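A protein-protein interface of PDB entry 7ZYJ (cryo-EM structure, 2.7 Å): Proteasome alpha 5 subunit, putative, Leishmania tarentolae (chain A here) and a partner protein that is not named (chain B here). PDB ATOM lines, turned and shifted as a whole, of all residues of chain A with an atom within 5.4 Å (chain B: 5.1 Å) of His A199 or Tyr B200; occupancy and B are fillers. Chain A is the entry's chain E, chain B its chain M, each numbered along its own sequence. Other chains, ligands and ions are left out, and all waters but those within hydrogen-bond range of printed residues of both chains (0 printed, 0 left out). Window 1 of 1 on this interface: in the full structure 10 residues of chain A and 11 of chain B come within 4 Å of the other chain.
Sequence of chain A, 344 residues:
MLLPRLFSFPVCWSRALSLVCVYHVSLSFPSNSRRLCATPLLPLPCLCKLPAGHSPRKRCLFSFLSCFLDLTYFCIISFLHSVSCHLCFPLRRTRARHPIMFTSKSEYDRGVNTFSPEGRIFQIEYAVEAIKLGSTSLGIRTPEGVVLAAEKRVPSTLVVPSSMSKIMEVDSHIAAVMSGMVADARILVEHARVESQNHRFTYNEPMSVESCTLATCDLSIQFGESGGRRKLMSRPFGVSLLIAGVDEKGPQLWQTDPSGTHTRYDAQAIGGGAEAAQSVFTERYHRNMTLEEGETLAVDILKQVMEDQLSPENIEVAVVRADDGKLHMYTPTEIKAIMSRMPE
Of chain B, only Tyr B200 (3.6 Å) comes within 4 Å of His A199.
Of the printed residues of chain B, Thr A202 touches Arg B196.
Of the printed residues of chain B, Tyr A203 touches Arg B196 and Tyr B200.
Printed residues of chain B within 4 Å of Glu A205: Tyr B200 and Lys B207.
Printed residues of chain B within 4 Å of Ser A208: Asn B204 (3.4 Å).
Lys B198 touches none of the printed residues of chain A.
Of chain A, only His A199 (3.6 Å), Tyr A203 (3.8 Å) and Glu A205 (2.3 Å) come within 4 Å of Tyr B200.
Lys B201 touches none of the printed residues of chain A.
The nearest residue of chain B that does not touch His A199 is Asn B204 (4.4 Å).
The nearest printed residue of chain A that does not touch Lys B207 is Ser A208 (7.4 Å).
OH of Tyr A203 lies within hydrogen-bond range of NH2 of Arg B196, 3.5 Å away.
OG of Ser A208 lies within hydrogen-bond range of ND2 of Asn B204 (3.4 Å).
The side-chain carboxylate (OE1) of Glu A205 lies within salt-bridge range of the side-chain amino group (NZ) of Lys B207, 3.99 Å away.
The side-chain hydroxyl (OH) of Tyr B200 sits close to the side-chain carboxylate (OE2) of Glu A205.
Tyr B200 touches His A199 (CE2 to NE2, 3.6 Å).
CG2 of Thr A202 touches NH2 of Arg B196 (3.8 Å).
Tyr A203 touches Tyr B200.
The backbone carbonyl oxygen of Tyr B200 lies close to the side-chain amide oxygen of Asn B204 (3.1 Å).
The side-chain hydroxyl (OG1) of Thr A202 lies within hydrogen-bond range of the backbone carbonyl oxygen (O) of Asn A198 (3.1 Å).
Hydrophobic or aromatic side chains of chain B within 4 Å of the printed part of chain A: Tyr B200.
Of the 15 printed residues of chain A, 5 touch a printed residue of chain B.
Hydrophobic or aromatic side chains of chain A that line the printed part of chain B: His A199 and Tyr A203.
Among the printed residues, 7 pairs touch across the chains.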
ATOM      1  N   VAL A 194      29.706  23.055  10.112  1.00  0.00           N
ATOM      2  CA  VAL A 194      28.840  24.213  10.313  1.00  0.00           C
ATOM      3  C   VAL A 194      27.945  24.009  11.529  1.00  0.00           C
ATOM      4  O   VAL A 194      27.769  24.918  12.348  1.00  0.00           O
ATOM      5  CB  VAL A 194      28.021  24.496   9.040  1.00  0.00           C
ATOM      6  CG1 VAL A 194      26.826  25.381   9.356  1.00  0.00           C
ATOM      7  CG2 VAL A 194      28.899  25.141   7.982  1.00  0.00           C
ATOM      8  N   GLU A 195      27.373  22.811  11.672  1.00  0.00           N
ATOM      9  CA  GLU A 195      26.499  22.545  12.810  1.00  0.00           C
ATOM     10  C   GLU A 195      27.271  22.557  14.124  1.00  0.00           C
ATOM     11  O   GLU A 195      26.767  23.053  15.138  1.00  0.00           O
ATOM     12  CB  GLU A 195      25.775  21.213  12.623  1.00  0.00           C
ATOM     13  CG  GLU A 195      24.845  21.184  11.426  1.00  0.00           C
ATOM     14  CD  GLU A 195      23.832  22.310  11.448  1.00  0.00           C
ATOM     15  OE1 GLU A 195      23.222  22.544  12.513  1.00  0.00           O
ATOM     16  OE2 GLU A 195      23.648  22.966  10.402  1.00  0.00           O
ATOM     17  N   SER A 196      28.490  22.014  14.132  1.00  0.00           N
ATOM     18  CA  SER A 196      29.300  22.038  15.346  1.00  0.00           C
ATOM     19  C   SER A 196      29.666  23.465  15.732  1.00  0.00           C
ATOM     20  O   SER A 196      29.639  23.825  16.917  1.00  0.00           O
ATOM     21  CB  SER A 196      30.555  21.190  15.154  1.00  0.00           C
ATOM     22  OG  SER A 196      31.358  21.194  16.320  1.00  0.00           O
ATOM     23  N   GLN A 197      30.004  24.297  14.745  1.00  0.00           N
ATOM     24  CA  GLN A 197      30.310  25.691  15.042  1.00  0.00           C
ATOM     25  C   GLN A 197      29.074  26.434  15.532  1.00  0.00           C
ATOM     26  O   GLN A 197      29.170  27.286  16.420  1.00  0.00           O
ATOM     27  CB  GLN A 197      30.907  26.371  13.813  1.00  0.00           C
ATOM     28  CG  GLN A 197      32.378  26.062  13.609  1.00  0.00           C
ATOM     29  CD  GLN A 197      33.171  26.141  14.898  1.00  0.00           C
ATOM     30  OE1 GLN A 197      33.266  27.200  15.518  1.00  0.00           O
ATOM     31  NE2 GLN A 197      33.738  25.016  15.313  1.00  0.00           N
ATOM     32  N   ASN A 198      27.903  26.118  14.973  1.00  0.00           N
ATOM     33  CA  ASN A 198      26.665  26.720  15.461  1.00  0.00           C
ATOM     34  C   ASN A 198      26.386  26.315  16.902  1.00  0.00           C
ATOM     35  O   ASN A 198      25.955  27.140  17.716  1.00  0.00           O
ATOM     36  CB  ASN A 198      25.498  26.321  14.560  1.00  0.00           C
ATOM     37  CG  ASN A 198      25.410  27.170  13.310  1.00  0.00           C
ATOM     38  OD1 ASN A 198      25.812  28.333  13.306  1.00  0.00           O
ATOM     39  ND2 ASN A 198      24.879  26.593  12.239  1.00  0.00           N
ATOM     40  N   HIS A 199      26.617  25.043  17.232  1.00  0.00           N
ATOM     41  CA  HIS A 199      26.418  24.583  18.602  1.00  0.00           C
ATOM     42  C   HIS A 199      27.373  25.281  19.562  1.00  0.00           C
ATOM     43  O   HIS A 199      26.978  25.673  20.666  1.00  0.00           O
ATOM     44  CB  HIS A 199      26.594  23.068  18.680  1.00  0.00           C
ATOM     45  CG  HIS A 199      26.148  22.476  19.979  1.00  0.00           C
ATOM     46  ND1 HIS A 199      26.958  22.432  21.093  1.00  0.00           N
ATOM     47  CD2 HIS A 199      24.977  21.906  20.345  1.00  0.00           C
ATOM     48  CE1 HIS A 199      26.306  21.858  22.087  1.00  0.00           C
ATOM     49  NE2 HIS A 199      25.101  21.529  21.660  1.00  0.00           N
ATOM     50  N   ARG A 200      28.638  25.438  19.162  1.00  0.00           N
ATOM     51  CA  ARG A 200      29.581  26.180  19.994  1.00  0.00           C
ATOM     52  C   ARG A 200      29.164  27.636  20.149  1.00  0.00           C
ATOM     53  O   ARG A 200      29.312  28.214  21.230  1.00  0.00           O
ATOM     54  CB  ARG A 200      30.990  26.096  19.407  1.00  0.00           C
ATOM     55  CG  ARG A 200      31.776  24.883  19.859  1.00  0.00           C
ATOM     56  CD  ARG A 200      33.227  24.982  19.432  1.00  0.00           C
ATOM     57  NE  ARG A 200      33.964  23.757  19.723  1.00  0.00           N
ATOM     58  CZ  ARG A 200      34.601  23.521  20.861  1.00  0.00           C
ATOM     59  NH1 ARG A 200      34.613  24.407  21.843  1.00  0.00           N
ATOM     60  NH2 ARG A 200      35.243  22.368  21.017  1.00  0.00           N
ATOM     61  N   PHE A 201      28.652  28.244  19.078  1.00  0.00           N
ATOM     62  CA  PHE A 201      28.213  29.633  19.137  1.00  0.00           C
ATOM     63  C   PHE A 201      27.031  29.806  20.082  1.00  0.00           C
ATOM     64  O   PHE A 201      26.977  30.778  20.845  1.00  0.00           O
ATOM     65  CB  PHE A 201      27.856  30.115  17.730  1.00  0.00           C
ATOM     66  CG  PHE A 201      27.373  31.533  17.676  1.00  0.00           C
ATOM     67  CD1 PHE A 201      28.267  32.573  17.512  1.00  0.00           C
ATOM     68  CD2 PHE A 201      26.023  31.826  17.770  1.00  0.00           C
ATOM     69  CE1 PHE A 201      27.828  33.877  17.459  1.00  0.00           C
ATOM     70  CE2 PHE A 201      25.580  33.129  17.718  1.00  0.00           C
ATOM     71  CZ  PHE A 201      26.484  34.156  17.562  1.00  0.00           C
ATOM     72  N   THR A 202      26.076  28.881  20.045  1.00  0.00           N
ATOM     73  CA  THR A 202      24.835  29.038  20.792  1.00  0.00           C
ATOM     74  C   THR A 202      24.954  28.600  22.246  1.00  0.00           C
ATOM     75  O   THR A 202      24.366  29.240  23.125  1.00  0.00           O
ATOM     76  CB  THR A 202      23.713  28.251  20.109  1.00  0.00           C
ATOM     77  OG1 THR A 202      23.524  28.748  18.777  1.00  0.00           O
ATOM     78  CG2 THR A 202      22.407  28.393  20.873  1.00  0.00           C
ATOM     79  N   TYR A 203      25.706  27.540  22.527  1.00  0.00           N
ATOM     80  CA  TYR A 203      25.755  26.963  23.862  1.00  0.00           C
ATOM     81  C   TYR A 203      27.107  27.116  24.545  1.00  0.00           C
ATOM     82  O   TYR A 203      27.241  26.717  25.706  1.00  0.00           O
ATOM     83  CB  TYR A 203      25.367  25.482  23.805  1.00  0.00           C
ATOM     84  CG  TYR A 203      23.995  25.252  23.218  1.00  0.00           C
ATOM     85  CD1 TYR A 203      22.850  25.526  23.953  1.00  0.00           C
ATOM     86  CD2 TYR A 203      23.845  24.779  21.924  1.00  0.00           C
ATOM     87  CE1 TYR A 203      21.595  25.324  23.419  1.00  0.00           C
ATOM     88  CE2 TYR A 203      22.594  24.573  21.381  1.00  0.00           C
ATOM     89  CZ  TYR A 203      21.473  24.848  22.132  1.00  0.00           C
ATOM     90  OH  TYR A 203      20.225  24.644  21.594  1.00  0.00           O
ATOM     91  N   ASN A 204      28.105  27.680  23.863  1.00  0.00           N
ATOM     92  CA  ASN A 204      29.429  27.921  24.443  1.00  0.00           C
ATOM     93  C   ASN A 204      30.028  26.636  25.014  1.00  0.00           C
ATOM     94  O   ASN A 204      30.599  26.616  26.106  1.00  0.00           O
ATOM     95  CB  ASN A 204      29.368  29.021  25.506  1.00  0.00           C
ATOM     96  CG  ASN A 204      30.738  29.542  25.887  1.00  0.00           C
ATOM     97  OD1 ASN A 204      31.688  29.444  25.113  1.00  0.00           O
ATOM     98  ND2 ASN A 204      30.847  30.097  27.087  1.00  0.00           N
ATOM     99  N   GLU A 205      29.888  25.549  24.261  1.00  0.00           N
ATOM    100  CA  GLU A 205      30.390  24.252  24.690  1.00  0.00           C
ATOM    101  C   GLU A 205      30.629  23.400  23.457  1.00  0.00           C
ATOM    102  O   GLU A 205      29.984  23.621  22.425  1.00  0.00           O
ATOM    103  CB  GLU A 205      29.398  23.562  25.636  1.00  0.00           C
ATOM    104  CG  GLU A 205      28.088  23.174  24.974  1.00  0.00           C
ATOM    105  CD  GLU A 205      27.319  22.143  25.766  1.00  0.00           C
ATOM    106  OE1 GLU A 205      27.687  21.891  26.932  1.00  0.00           O
ATOM    107  OE2 GLU A 205      26.346  21.580  25.223  1.00  0.00           O
ATOM    108  N   PRO A 206      31.550  22.440  23.517  1.00  0.00           N
ATOM    109  CA  PRO A 206      31.737  21.534  22.379  1.00  0.00           C
ATOM    110  C   PRO A 206      30.492  20.700  22.130  1.00  0.00           C
ATOM    111  O   PRO A 206      29.808  20.274  23.064  1.00  0.00           O
ATOM    112  CB  PRO A 206      32.924  20.662  22.805  1.00  0.00           C
ATOM    113  CG  PRO A 206      32.962  20.766  24.290  1.00  0.00           C
ATOM    114  CD  PRO A 206      32.484  22.145  24.617  1.00  0.00           C
ATOM    115  N   MET A 207      30.203  20.468  20.853  1.00  0.00           N
ATOM    116  CA  MET A 207      29.022  19.705  20.485  1.00  0.00           C
ATOM    117  C   MET A 207      29.302  18.213  20.623  1.00  0.00           C
ATOM    118  O   MET A 207      30.386  17.728  20.289  1.00  0.00           O
ATOM    119  CB  MET A 207      28.605  20.049  19.054  1.00  0.00           C
ATOM    120  CG  MET A 207      27.332  19.387  18.563  1.00  0.00           C
ATOM    121  SD  MET A 207      26.941  19.977  16.905  1.00  0.00           S
ATOM    122  CE  MET A 207      25.497  19.016  16.494  1.00  0.00           C
ATOM    123  N   SER A 208      28.314  17.484  21.130  1.00  0.00           N
ATOM    124  CA  SER A 208      28.479  16.056  21.358  1.00  0.00           C
ATOM    125  C   SER A 208      28.582  15.308  20.036  1.00  0.00           C
ATOM    126  O   SER A 208      28.086  15.760  18.999  1.00  0.00           O
ATOM    127  CB  SER A 208      27.317  15.504  22.184  1.00  0.00           C
ATOM    128  OG  SER A 208      26.144  15.386  21.399  1.00  0.00           O
ATOM    129  N   TYR B 195      11.312  25.310  25.957  1.00  0.00           N
ATOM    130  CA  TYR B 195      11.256  24.437  24.793  1.00  0.00           C
ATOM    131  C   TYR B 195      12.621  24.260  24.139  1.00  0.00           C
ATOM    132  O   TYR B 195      12.916  23.173  23.631  1.00  0.00           O
ATOM    133  CB  TYR B 195      10.221  24.962  23.800  1.00  0.00           C
ATOM    134  CG  TYR B 195       8.813  24.777  24.317  1.00  0.00           C
ATOM    135  CD1 TYR B 195       8.439  23.588  24.930  1.00  0.00           C
ATOM    136  CD2 TYR B 195       7.868  25.788  24.215  1.00  0.00           C
ATOM    137  CE1 TYR B 195       7.162  23.405  25.415  1.00  0.00           C
ATOM    138  CE2 TYR B 195       6.585  25.613  24.700  1.00  0.00           C
ATOM    139  CZ  TYR B 195       6.239  24.418  25.299  1.00  0.00           C
ATOM    140  OH  TYR B 195       4.966  24.232  25.784  1.00  0.00           O
ATOM    141  N   ARG B 196      13.475  25.286  24.167  1.00  0.00           N
ATOM    142  CA  ARG B 196      14.841  25.106  23.685  1.00  0.00           C
ATOM    143  C   ARG B 196      15.609  24.116  24.554  1.00  0.00           C
ATOM    144  O   ARG B 196      16.376  23.294  24.041  1.00  0.00           O
ATOM    145  CB  ARG B 196      15.562  26.451  23.632  1.00  0.00           C
ATOM    146  CG  ARG B 196      15.113  27.336  22.490  1.00  0.00           C
ATOM    147  CD  ARG B 196      15.418  26.702  21.146  1.00  0.00           C
ATOM    148  NE  ARG B 196      16.851  26.648  20.885  1.00  0.00           N
ATOM    149  CZ  ARG B 196      17.529  27.584  20.235  1.00  0.00           C
ATOM    150  NH1 ARG B 196      16.933  28.666  19.763  1.00  0.00           N
ATOM    151  NH2 ARG B 196      18.836  27.431  20.055  1.00  0.00           N
ATOM    152  N   VAL B 197      15.414  24.178  25.872  1.00  0.00           N
ATOM    153  CA  VAL B 197      16.067  23.231  26.771  1.00  0.00           C
ATOM    154  C   VAL B 197      15.566  21.816  26.512  1.00  0.00           C
ATOM    155  O   VAL B 197      16.344  20.854  26.519  1.00  0.00           O
ATOM    156  CB  VAL B 197      15.849  23.656  28.235  1.00  0.00           C
ATOM    157  CG1 VAL B 197      16.185  22.518  29.185  1.00  0.00           C
ATOM    158  CG2 VAL B 197      16.689  24.880  28.559  1.00  0.00           C
ATOM    159  N   LYS B 198      14.262  21.664  26.280  1.00  0.00           N
ATOM    160  CA  LYS B 198      13.713  20.343  25.993  1.00  0.00           C
ATOM    161  C   LYS B 198      14.245  19.798  24.669  1.00  0.00           C
ATOM    162  O   LYS B 198      14.556  18.605  24.558  1.00  0.00           O
ATOM    163  CB  LYS B 198      12.187  20.417  25.993  1.00  0.00           C
ATOM    164  CG  LYS B 198      11.475  19.094  25.819  1.00  0.00           C
ATOM    165  CD  LYS B 198       9.972  19.296  25.926  1.00  0.00           C
ATOM    166  CE  LYS B 198       9.216  17.994  25.751  1.00  0.00           C
ATOM    167  NZ  LYS B 198       7.744  18.188  25.852  1.00  0.00           N
ATOM    168  N   TRP B 199      14.375  20.663  23.657  1.00  0.00           N
ATOM    169  CA  TRP B 199      14.981  20.244  22.398  1.00  0.00           C
ATOM    170  C   TRP B 199      16.438  19.839  22.590  1.00  0.00           C
ATOM    171  O   TRP B 199      16.902  18.863  21.991  1.00  0.00           O
ATOM    172  CB  TRP B 199      14.873  21.361  21.360  1.00  0.00           C
ATOM    173  CG  TRP B 199      13.619  21.325  20.534  1.00  0.00           C
ATOM    174  CD1 TRP B 199      12.772  22.365  20.296  1.00  0.00           C
ATOM    175  CD2 TRP B 199      13.085  20.202  19.818  1.00  0.00           C
ATOM    176  NE1 TRP B 199      11.738  21.960  19.489  1.00  0.00           N
ATOM    177  CE2 TRP B 199      11.908  20.636  19.181  1.00  0.00           C
ATOM    178  CE3 TRP B 199      13.486  18.871  19.657  1.00  0.00           C
ATOM    179  CZ2 TRP B 199      11.126  19.790  18.398  1.00  0.00           C
ATOM    180  CZ3 TRP B 199      12.709  18.033  18.881  1.00  0.00           C
ATOM    181  CH2 TRP B 199      11.544  18.496  18.261  1.00  0.00           C
ATOM    182  N   TYR B 200      17.179  20.588  23.409  1.00  0.00           N
ATOM    183  CA  TYR B 200      18.561  20.227  23.705  1.00  0.00           C
ATOM    184  C   TYR B 200      18.632  18.860  24.373  1.00  0.00           C
ATOM    185  O   TYR B 200      19.502  18.042  24.054  1.00  0.00           O
ATOM    186  CB  TYR B 200      19.203  21.301  24.588  1.00  0.00           C
ATOM    187  CG  TYR B 200      20.649  21.042  24.963  1.00  0.00           C
ATOM    188  CD1 TYR B 200      20.977  20.198  26.016  1.00  0.00           C
ATOM    189  CD2 TYR B 200      21.683  21.648  24.265  1.00  0.00           C
ATOM    190  CE1 TYR B 200      22.291  19.961  26.358  1.00  0.00           C
ATOM    191  CE2 TYR B 200      23.003  21.417  24.601  1.00  0.00           C
ATOM    192  CZ  TYR B 200      23.300  20.573  25.649  1.00  0.00           C
ATOM    193  OH  TYR B 200      24.610  20.340  25.990  1.00  0.00           O
ATOM    194  N   LYS B 201      17.726  18.604  25.316  1.00  0.00           N
ATOM    195  CA  LYS B 201      17.694  17.306  25.983  1.00  0.00           C
ATOM    196  C   LYS B 201      17.394  16.188  24.992  1.00  0.00           C
ATOM    197  O   LYS B 201      17.988  15.106  25.065  1.00  0.00           O
ATOM    198  CB  LYS B 201      16.661  17.325  27.109  1.00  0.00           C
ATOM    199  CG  LYS B 201      16.343  15.961  27.690  1.00  0.00           C
ATOM    200  CD  LYS B 201      15.590  16.084  29.002  1.00  0.00           C
ATOM    201  CE  LYS B 201      16.422  16.802  30.050  1.00  0.00           C
ATOM    202  NZ  LYS B 201      15.724  16.869  31.362  1.00  0.00           N
ATOM    203  N   TYR B 202      16.473  16.432  24.057  1.00  0.00           N
ATOM    204  CA  TYR B 202      16.184  15.437  23.028  1.00  0.00           C
ATOM    205  C   TYR B 202      17.386  15.191  22.124  1.00  0.00           C
ATOM    206  O   TYR B 202      17.665  14.045  21.753  1.00  0.00           O
ATOM    207  CB  TYR B 202      14.977  15.871  22.197  1.00  0.00           C
ATOM    208  CG  TYR B 202      13.658  15.679  22.900  1.00  0.00           C
ATOM    209  CD1 TYR B 202      13.503  14.682  23.850  1.00  0.00           C
ATOM    210  CD2 TYR B 202      12.566  16.482  22.605  1.00  0.00           C
ATOM    211  CE1 TYR B 202      12.304  14.494  24.492  1.00  0.00           C
ATOM    212  CE2 TYR B 202      11.358  16.301  23.246  1.00  0.00           C
ATOM    213  CZ  TYR B 202      11.234  15.303  24.188  1.00  0.00           C
ATOM    214  OH  TYR B 202      10.035  15.109  24.834  1.00  0.00           O
ATOM    215  N   ASN B 203      18.106  16.250  21.755  1.00  0.00           N
ATOM    216  CA  ASN B 203      19.183  16.129  20.781  1.00  0.00           C
ATOM    217  C   ASN B 203      20.508  15.699  21.398  1.00  0.00           C
ATOM    218  O   ASN B 203      21.470  15.470  20.658  1.00  0.00           O
ATOM    219  CB  ASN B 203      19.374  17.455  20.042  1.00  0.00           C
ATOM    220  CG  ASN B 203      18.218  17.778  19.119  1.00  0.00           C
ATOM    221  OD1 ASN B 203      17.511  16.884  18.657  1.00  0.00           O
ATOM    222  ND2 ASN B 203      18.020  19.061  18.845  1.00  0.00           N
ATOM    223  N   ASN B 204      20.587  15.583  22.720  1.00  0.00           N
ATOM    224  CA  ASN B 204      21.825  15.231  23.404  1.00  0.00           C
ATOM    225  C   ASN B 204      21.640  14.004  24.289  1.00  0.00           C
ATOM    226  O   ASN B 204      22.320  13.838  25.302  1.00  0.00           O
ATOM    227  CB  ASN B 204      22.348  16.413  24.217  1.00  0.00           C
ATOM    228  CG  ASN B 204      22.979  17.481  23.348  1.00  0.00           C
ATOM    229  OD1 ASN B 204      22.286  18.306  22.753  1.00  0.00           O
ATOM    230  ND2 ASN B 204      24.305  17.472  23.271  1.00  0.00           N
ATOM    231  N   GLY B 205      20.717  13.126  23.906  1.00  0.00           N
ATOM    232  CA  GLY B 205      20.519  11.883  24.626  1.00  0.00           C
ATOM    233  C   GLY B 205      20.071  12.039  26.061  1.00  0.00           C
ATOM    234  O   GLY B 205      20.536  11.297  26.932  1.00  0.00           O
ATOM    235  N   LYS B 207      20.735  14.484  28.062  1.00  0.00           N
ATOM    236  CA  LYS B 207      21.686  15.237  28.867  1.00  0.00           C
ATOM    237  C   LYS B 207      21.144  16.642  29.093  1.00  0.00           C
ATOM    238  O   LYS B 207      20.862  17.369  28.135  1.00  0.00           O
ATOM    239  CB  LYS B 207      23.050  15.266  28.176  1.00  0.00           C
ATOM    240  CG  LYS B 207      24.188  15.872  28.991  1.00  0.00           C
ATOM    241  CD  LYS B 207      24.343  17.365  28.744  1.00  0.00           C
ATOM    242  CE  LYS B 207      25.527  17.929  29.508  1.00  0.00           C
ATOM    243  NZ  LYS B 207      25.672  19.396  29.306  1.00  0.00           N
ATOM    244  N   VAL B 208      20.991  17.020  30.356  1.00  0.00           N
ATOM    245  CA  VAL B 208      20.426  18.333  30.686  1.00  0.00           C
ATOM    246  C   VAL B 208      21.481  19.409  30.449  1.00  0.00           C
ATOM    247  O   VAL B 208      22.666  19.189  30.759  1.00  0.00           O
ATOM    248  CB  VAL B 208      19.915  18.342  32.135  1.00  0.00           C
ATOM    249  CG1 VAL B 208      21.055  18.438  33.146  1.00  0.00           C
ATOM    250  CG2 VAL B 208      18.902  19.449  32.351  1.00  0.00           C
ATOM    251  N   PRO B 209      21.129  20.550  29.861  1.00  0.00           N
ATOM    252  CA  PRO B 209      22.131  21.591  29.614  1.00  0.00           C
ATOM    253  C   PRO B 209      22.653  22.197  30.908  1.00  0.00           C
ATOM    254  O   PRO B 209      21.961  22.265  31.927  1.00  0.00           O
ATOM    255  CB  PRO B 209      21.375  22.631  28.780  1.00  0.00           C
ATOM    256  CG  PRO B 209      19.937  22.379  29.063  1.00  0.00           C
ATOM    257  CD  PRO B 209      19.815  20.906  29.299  1.00  0.00           C
